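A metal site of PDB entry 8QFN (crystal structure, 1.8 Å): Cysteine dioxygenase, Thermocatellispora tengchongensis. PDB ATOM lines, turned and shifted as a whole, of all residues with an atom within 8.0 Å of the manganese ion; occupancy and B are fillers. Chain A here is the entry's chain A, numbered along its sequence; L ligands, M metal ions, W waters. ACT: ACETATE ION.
ND1 of His 134 sits at hydrogen-bond distance from OE1 of Glu 106. The backbone carbonyl oxygen (O) of Gly 86 lies within hydrogen-bond range of a ring nitrogen (ND1) of His 88 (3.0 Å).
The nearest printed residue that does not touch the manganese ion is Tyr 149 (4.01 Å).
The manganese ion is bound by a ring nitrogen (NE2) of His 134, at 2.1 Å. The manganese ion is bound by a ring nitrogen (NE2) of His 90 (2.1 Å). Water W1 binds the manganese ion. The manganese ion is bound by NE2 of His 88 (2.1 Å). O of the ligand is bound to the manganese ion. The manganese ion is bound by water W2. The manganese ion has six donor atoms within binding distance.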
ATOM      1  N   LEU A  77     -31.905   2.947  15.060  1.00  0.00           N
ATOM      2  CA  LEU A  77     -32.825   3.054  16.177  1.00  0.00           C
ATOM      3  C   LEU A  77     -33.771   4.227  15.961  1.00  0.00           C
ATOM      4  O   LEU A  77     -33.337   5.337  15.629  1.00  0.00           O
ATOM      5  CB  LEU A  77     -32.059   3.233  17.492  1.00  0.00           C
ATOM      6  CG  LEU A  77     -31.659   1.953  18.233  1.00  0.00           C
ATOM      7  CD1 LEU A  77     -30.855   1.034  17.321  1.00  0.00           C
ATOM      8  CD2 LEU A  77     -30.872   2.272  19.506  1.00  0.00           C
ATOM      9  N   THR A  85     -32.419   2.945  27.362  1.00  0.00           N
ATOM     10  CA  THR A  85     -31.614   1.743  27.250  1.00  0.00           C
ATOM     11  C   THR A  85     -31.368   1.101  28.608  1.00  0.00           C
ATOM     12  O   THR A  85     -31.071  -0.091  28.674  1.00  0.00           O
ATOM     13  CB  THR A  85     -30.252   2.025  26.622  1.00  0.00           C
ATOM     14  OG1 THR A  85     -29.517   2.940  27.448  1.00  0.00           O
ATOM     15  CG2 THR A  85     -30.397   2.588  25.223  1.00  0.00           C
ATOM     16  N   GLY A  86     -31.454   1.881  29.676  1.00  0.00           N
ATOM     17  CA  GLY A  86     -30.917   1.457  30.961  1.00  0.00           C
ATOM     18  C   GLY A  86     -29.410   1.610  30.967  1.00  0.00           C
ATOM     19  O   GLY A  86     -28.792   1.847  29.923  1.00  0.00           O
ATOM     20  N   TRP A  87     -28.807   1.468  32.137  1.00  0.00           N
ATOM     21  CA  TRP A  87     -27.357   1.519  32.249  1.00  0.00           C
ATOM     22  C   TRP A  87     -26.755   0.217  31.755  1.00  0.00           C
ATOM     23  O   TRP A  87     -27.227  -0.869  32.129  1.00  0.00           O
ATOM     24  CB  TRP A  87     -26.956   1.752  33.702  1.00  0.00           C
ATOM     25  CG  TRP A  87     -27.375   3.068  34.262  1.00  0.00           C
ATOM     26  CD1 TRP A  87     -28.405   3.310  35.112  1.00  0.00           C
ATOM     27  CD2 TRP A  87     -26.742   4.328  34.025  1.00  0.00           C
ATOM     28  NE1 TRP A  87     -28.454   4.641  35.431  1.00  0.00           N
ATOM     29  CE2 TRP A  87     -27.450   5.297  34.770  1.00  0.00           C
ATOM     30  CE3 TRP A  87     -25.652   4.737  33.248  1.00  0.00           C
ATOM     31  CZ2 TRP A  87     -27.100   6.639  34.768  1.00  0.00           C
ATOM     32  CZ3 TRP A  87     -25.303   6.079  33.246  1.00  0.00           C
ATOM     33  CH2 TRP A  87     -26.027   7.009  33.993  1.00  0.00           C
ATOM     34  N   HIS A  88     -25.745   0.302  30.896  1.00  0.00           N
ATOM     35  CA  HIS A  88     -25.181  -0.916  30.329  1.00  0.00           C
ATOM     36  C   HIS A  88     -23.768  -0.658  29.829  1.00  0.00           C
ATOM     37  O   HIS A  88     -23.366   0.471  29.575  1.00  0.00           O
ATOM     38  CB  HIS A  88     -26.035  -1.422  29.188  1.00  0.00           C
ATOM     39  CG  HIS A  88     -26.065  -0.504  28.003  1.00  0.00           C
ATOM     40  ND1 HIS A  88     -26.909   0.587  27.938  1.00  0.00           N
ATOM     41  CD2 HIS A  88     -25.327  -0.475  26.869  1.00  0.00           C
ATOM     42  CE1 HIS A  88     -26.704   1.229  26.798  1.00  0.00           C
ATOM     43  NE2 HIS A  88     -25.752   0.598  26.131  1.00  0.00           N
ATOM     44  N   ASP A  89     -23.021  -1.756  29.698  1.00  0.00           N
ATOM     45  CA  ASP A  89     -21.767  -1.787  28.975  1.00  0.00           C
ATOM     46  C   ASP A  89     -21.927  -2.718  27.791  1.00  0.00           C
ATOM     47  O   ASP A  89     -22.947  -3.414  27.633  1.00  0.00           O
ATOM     48  CB  ASP A  89     -20.607  -2.259  29.875  1.00  0.00           C
ATOM     49  CG  ASP A  89     -20.800  -3.668  30.372  1.00  0.00           C
ATOM     50  OD1 ASP A  89     -20.740  -4.598  29.539  1.00  0.00           O
ATOM     51  OD2 ASP A  89     -20.997  -3.854  31.589  1.00  0.00           O
ATOM     52  N   HIS A  90     -20.901  -2.742  26.937  1.00  0.00           N
ATOM     53  CA  HIS A  90     -20.912  -3.539  25.723  1.00  0.00           C
ATOM     54  C   HIS A  90     -19.860  -4.632  25.756  1.00  0.00           C
ATOM     55  O   HIS A  90     -19.430  -5.114  24.709  1.00  0.00           O
ATOM     56  CB  HIS A  90     -20.730  -2.597  24.533  1.00  0.00           C
ATOM     57  CG  HIS A  90     -21.565  -1.354  24.637  1.00  0.00           C
ATOM     58  ND1 HIS A  90     -21.100  -0.175  25.172  1.00  0.00           N
ATOM     59  CD2 HIS A  90     -22.857  -1.129  24.311  1.00  0.00           C
ATOM     60  CE1 HIS A  90     -22.064   0.730  25.140  1.00  0.00           C
ATOM     61  NE2 HIS A  90     -23.136   0.178  24.621  1.00  0.00           N
ATOM     62  N   GLY A  95     -17.865   1.207  20.234  1.00  0.00           N
ATOM     63  CA  GLY A  95     -19.118   1.649  19.663  1.00  0.00           C
ATOM     64  C   GLY A  95     -19.106   3.090  19.210  1.00  0.00           C
ATOM     65  O   GLY A  95     -18.246   3.879  19.615  1.00  0.00           O
ATOM     66  N   ALA A  96     -20.071   3.431  18.362  1.00  0.00           N
ATOM     67  CA  ALA A  96     -20.280   4.818  17.973  1.00  0.00           C
ATOM     68  C   ALA A  96     -21.743   5.064  17.677  1.00  0.00           C
ATOM     69  O   ALA A  96     -22.500   4.158  17.304  1.00  0.00           O
ATOM     70  CB  ALA A  96     -19.410   5.193  16.755  1.00  0.00           C
ATOM     71  N   VAL A  97     -22.135   6.316  17.843  1.00  0.00           N
ATOM     72  CA  VAL A  97     -23.515   6.764  17.664  1.00  0.00           C
ATOM     73  C   VAL A  97     -23.507   8.020  16.809  1.00  0.00           C
ATOM     74  O   VAL A  97     -22.694   8.931  17.018  1.00  0.00           O
ATOM     75  CB  VAL A  97     -24.200   7.065  19.015  1.00  0.00           C
ATOM     76  CG1 VAL A  97     -25.608   7.576  18.783  1.00  0.00           C
ATOM     77  CG2 VAL A  97     -24.187   5.834  19.910  1.00  0.00           C
ATOM     78  N   GLU A 106     -27.007  11.241  26.250  1.00  0.00           N
ATOM     79  CA  GLU A 106     -25.970  10.278  26.595  1.00  0.00           C
ATOM     80  C   GLU A 106     -25.610  10.496  28.058  1.00  0.00           C
ATOM     81  O   GLU A 106     -25.186  11.593  28.435  1.00  0.00           O
ATOM     82  CB  GLU A 106     -24.747  10.450  25.685  1.00  0.00           C
ATOM     83  CG  GLU A 106     -23.404   9.983  26.284  1.00  0.00           C
ATOM     84  CD  GLU A 106     -23.187   8.484  26.127  1.00  0.00           C
ATOM     85  OE1 GLU A 106     -24.169   7.774  25.848  1.00  0.00           O
ATOM     86  OE2 GLU A 106     -22.023   8.027  26.283  1.00  0.00           O
ATOM     87  N   PHE A 126     -20.604  10.464  18.510  1.00  0.00           N
ATOM     88  CA  PHE A 126     -19.537  10.186  19.459  1.00  0.00           C
ATOM     89  C   PHE A 126     -19.206   8.700  19.391  1.00  0.00           C
ATOM     90  O   PHE A 126     -19.982   7.895  18.871  1.00  0.00           O
ATOM     91  CB  PHE A 126     -19.927  10.606  20.897  1.00  0.00           C
ATOM     92  CG  PHE A 126     -21.106   9.858  21.452  1.00  0.00           C
ATOM     93  CD1 PHE A 126     -22.396  10.245  21.168  1.00  0.00           C
ATOM     94  CD2 PHE A 126     -20.909   8.767  22.295  1.00  0.00           C
ATOM     95  CE1 PHE A 126     -23.487   9.563  21.683  1.00  0.00           C
ATOM     96  CE2 PHE A 126     -21.982   8.083  22.809  1.00  0.00           C
ATOM     97  CZ  PHE A 126     -23.266   8.477  22.510  1.00  0.00           C
ATOM     98  N   PHE A 128     -16.790   5.406  21.580  1.00  0.00           N
ATOM     99  CA  PHE A 128     -16.238   5.009  22.870  1.00  0.00           C
ATOM    100  C   PHE A 128     -15.568   3.654  22.697  1.00  0.00           C
ATOM    101  O   PHE A 128     -15.903   2.886  21.800  1.00  0.00           O
ATOM    102  CB  PHE A 128     -17.319   4.935  23.943  1.00  0.00           C
ATOM    103  CG  PHE A 128     -18.542   4.175  23.522  1.00  0.00           C
ATOM    104  CD1 PHE A 128     -18.542   2.788  23.526  1.00  0.00           C
ATOM    105  CD2 PHE A 128     -19.680   4.833  23.094  1.00  0.00           C
ATOM    106  CE1 PHE A 128     -19.642   2.081  23.129  1.00  0.00           C
ATOM    107  CE2 PHE A 128     -20.792   4.123  22.690  1.00  0.00           C
ATOM    108  CZ  PHE A 128     -20.772   2.760  22.707  1.00  0.00           C
ATOM    109  N   HIS A 132     -16.658   1.416  28.188  1.00  0.00           N
ATOM    110  CA  HIS A 132     -17.707   2.412  28.358  1.00  0.00           C
ATOM    111  C   HIS A 132     -18.925   1.859  29.088  1.00  0.00           C
ATOM    112  O   HIS A 132     -19.417   0.773  28.783  1.00  0.00           O
ATOM    113  CB  HIS A 132     -18.125   2.924  26.967  1.00  0.00           C
ATOM    114  CG  HIS A 132     -18.825   4.240  26.959  1.00  0.00           C
ATOM    115  ND1 HIS A 132     -18.235   5.407  27.393  1.00  0.00           N
ATOM    116  CD2 HIS A 132     -20.051   4.598  26.497  1.00  0.00           C
ATOM    117  CE1 HIS A 132     -19.072   6.419  27.232  1.00  0.00           C
ATOM    118  NE2 HIS A 132     -20.185   5.957  26.688  1.00  0.00           N
ATOM    119  N   ILE A 133     -19.426   2.629  30.059  1.00  0.00           N
ATOM    120  CA  ILE A 133     -20.720   2.380  30.683  1.00  0.00           C
ATOM    121  C   ILE A 133     -21.598   3.596  30.400  1.00  0.00           C
ATOM    122  O   ILE A 133     -21.200   4.725  30.691  1.00  0.00           O
ATOM    123  CB  ILE A 133     -20.604   2.148  32.208  1.00  0.00           C
ATOM    124  CG1 ILE A 133     -19.722   0.960  32.546  1.00  0.00           C
ATOM    125  CG2 ILE A 133     -22.033   1.991  32.781  1.00  0.00           C
ATOM    126  CD1 ILE A 133     -19.363   0.871  34.031  1.00  0.00           C
ATOM    127  N   HIS A 134     -22.789   3.366  29.875  1.00  0.00           N
ATOM    128  CA  HIS A 134     -23.630   4.516  29.523  1.00  0.00           C
ATOM    129  C   HIS A 134     -25.110   4.137  29.514  1.00  0.00           C
ATOM    130  O   HIS A 134     -25.498   2.991  29.719  1.00  0.00           O
ATOM    131  CB  HIS A 134     -23.186   5.133  28.189  1.00  0.00           C
ATOM    132  CG  HIS A 134     -23.645   4.387  26.967  1.00  0.00           C
ATOM    133  ND1 HIS A 134     -23.895   5.017  25.758  1.00  0.00           N
ATOM    134  CD2 HIS A 134     -23.877   3.074  26.745  1.00  0.00           C
ATOM    135  CE1 HIS A 134     -24.279   4.131  24.867  1.00  0.00           C
ATOM    136  NE2 HIS A 134     -24.272   2.937  25.428  1.00  0.00           N
ATOM    137  N   ARG A 135     -25.928   5.169  29.309  1.00  0.00           N
ATOM    138  CA  ARG A 135     -27.376   5.078  29.214  1.00  0.00           C
ATOM    139  C   ARG A 135     -27.821   6.111  28.202  1.00  0.00           C
ATOM    140  O   ARG A 135     -27.389   7.261  28.258  1.00  0.00           O
ATOM    141  CB  ARG A 135     -28.025   5.334  30.580  1.00  0.00           C
ATOM    142  CG  ARG A 135     -29.515   5.273  30.563  1.00  0.00           C
ATOM    143  CD  ARG A 135     -30.026   5.462  31.965  1.00  0.00           C
ATOM    144  NE  ARG A 135     -31.427   5.807  31.975  1.00  0.00           N
ATOM    145  CZ  ARG A 135     -32.003   6.536  32.921  1.00  0.00           C
ATOM    146  NH1 ARG A 135     -31.300   7.008  33.946  1.00  0.00           N
ATOM    147  NH2 ARG A 135     -33.310   6.804  32.841  1.00  0.00           N
ATOM    148  N   LEU A 136     -28.656   5.694  27.254  1.00  0.00           N
ATOM    149  CA  LEU A 136     -29.254   6.600  26.294  1.00  0.00           C
ATOM    150  C   LEU A 136     -30.735   6.726  26.592  1.00  0.00           C
ATOM    151  O   LEU A 136     -31.440   5.711  26.698  1.00  0.00           O
ATOM    152  CB  LEU A 136     -29.039   6.122  24.854  1.00  0.00           C
ATOM    153  CG  LEU A 136     -27.603   6.088  24.325  1.00  0.00           C
ATOM    154  CD1 LEU A 136     -27.602   5.458  22.940  1.00  0.00           C
ATOM    155  CD2 LEU A 136     -27.003   7.486  24.295  1.00  0.00           C
ATOM    156  N   HIS A 147     -26.188   3.208  15.114  1.00  0.00           N
ATOM    157  CA  HIS A 147     -25.281   2.690  16.134  1.00  0.00           C
ATOM    158  C   HIS A 147     -24.455   1.571  15.543  1.00  0.00           C
ATOM    159  O   HIS A 147     -25.013   0.658  14.919  1.00  0.00           O
ATOM    160  CB  HIS A 147     -26.061   2.193  17.349  1.00  0.00           C
ATOM    161  CG  HIS A 147     -26.993   3.204  17.926  1.00  0.00           C
ATOM    162  ND1 HIS A 147     -26.880   3.672  19.211  1.00  0.00           N
ATOM    163  CD2 HIS A 147     -28.059   3.843  17.378  1.00  0.00           C
ATOM    164  CE1 HIS A 147     -27.831   4.556  19.448  1.00  0.00           C
ATOM    165  NE2 HIS A 147     -28.563   4.684  18.352  1.00  0.00           N
ATOM    166  N   TYR A 149     -21.034  -1.214  16.286  1.00  0.00           N
ATOM    167  CA  TYR A 149     -20.246  -1.896  17.296  1.00  0.00           C
ATOM    168  C   TYR A 149     -19.194  -2.765  16.631  1.00  0.00           C
ATOM    169  O   TYR A 149     -19.485  -3.444  15.643  1.00  0.00           O
ATOM    170  CB  TYR A 149     -21.132  -2.764  18.184  1.00  0.00           C
ATOM    171  CG  TYR A 149     -22.269  -2.022  18.821  1.00  0.00           C
ATOM    172  CD1 TYR A 149     -22.135  -1.468  20.073  1.00  0.00           C
ATOM    173  CD2 TYR A 149     -23.486  -1.861  18.149  1.00  0.00           C
ATOM    174  CE1 TYR A 149     -23.180  -0.785  20.661  1.00  0.00           C
ATOM    175  CE2 TYR A 149     -24.520  -1.176  18.731  1.00  0.00           C
ATOM    176  CZ  TYR A 149     -24.364  -0.640  19.983  1.00  0.00           C
ATOM    177  OH  TYR A 149     -25.410   0.042  20.557  1.00  0.00           O
ATOM    178  N   LEU A 153     -21.662  -6.764  18.900  1.00  0.00           N
ATOM    179  CA  LEU A 153     -22.377  -6.711  20.164  1.00  0.00           C
ATOM    180  C   LEU A 153     -23.089  -8.049  20.385  1.00  0.00           C
ATOM    181  O   LEU A 153     -24.310  -8.183  20.273  1.00  0.00           O
ATOM    182  CB  LEU A 153     -23.369  -5.550  20.155  1.00  0.00           C
ATOM    183  CG  LEU A 153     -24.019  -5.201  21.481  1.00  0.00           C
ATOM    184  CD1 LEU A 153     -22.948  -4.764  22.473  1.00  0.00           C
ATOM    185  CD2 LEU A 153     -25.056  -4.106  21.285  1.00  0.00           C
ATOM    186  N   LEU A 156     -23.765  -7.941  26.241  1.00  0.00           N
ATOM    187  CA  LEU A 156     -23.763  -6.671  26.944  1.00  0.00           C
ATOM    188  C   LEU A 156     -24.100  -6.890  28.413  1.00  0.00           C
ATOM    189  O   LEU A 156     -24.717  -7.884  28.799  1.00  0.00           O
ATOM    190  CB  LEU A 156     -24.710  -5.658  26.325  1.00  0.00           C
ATOM    191  CG  LEU A 156     -26.199  -5.899  26.266  1.00  0.00           C
ATOM    192  CD1 LEU A 156     -26.846  -5.367  27.534  1.00  0.00           C
ATOM    193  CD2 LEU A 156     -26.778  -5.244  25.027  1.00  0.00           C
HETATM  194  C   ACT L   1     -24.275   2.475  21.464  1.00  0.00           C
HETATM  195  O   ACT L   1     -24.016   1.838  22.482  1.00  0.00           O
HETATM  196  OXT ACT L   1     -25.430   3.145  21.390  1.00  0.00           O
HETATM  197  CH3 ACT L   1     -23.454   2.625  20.230  1.00  0.00           C
HETATM  198 MN    MN M   1     -24.882   1.285  24.338  1.00  0.00          MN
HETATM  199  O   HOH W   1     -25.747  -0.270  23.249  1.00  0.00           O
HETATM  200  O   HOH W   2     -26.761   2.339  23.679  1.00  0.00           O
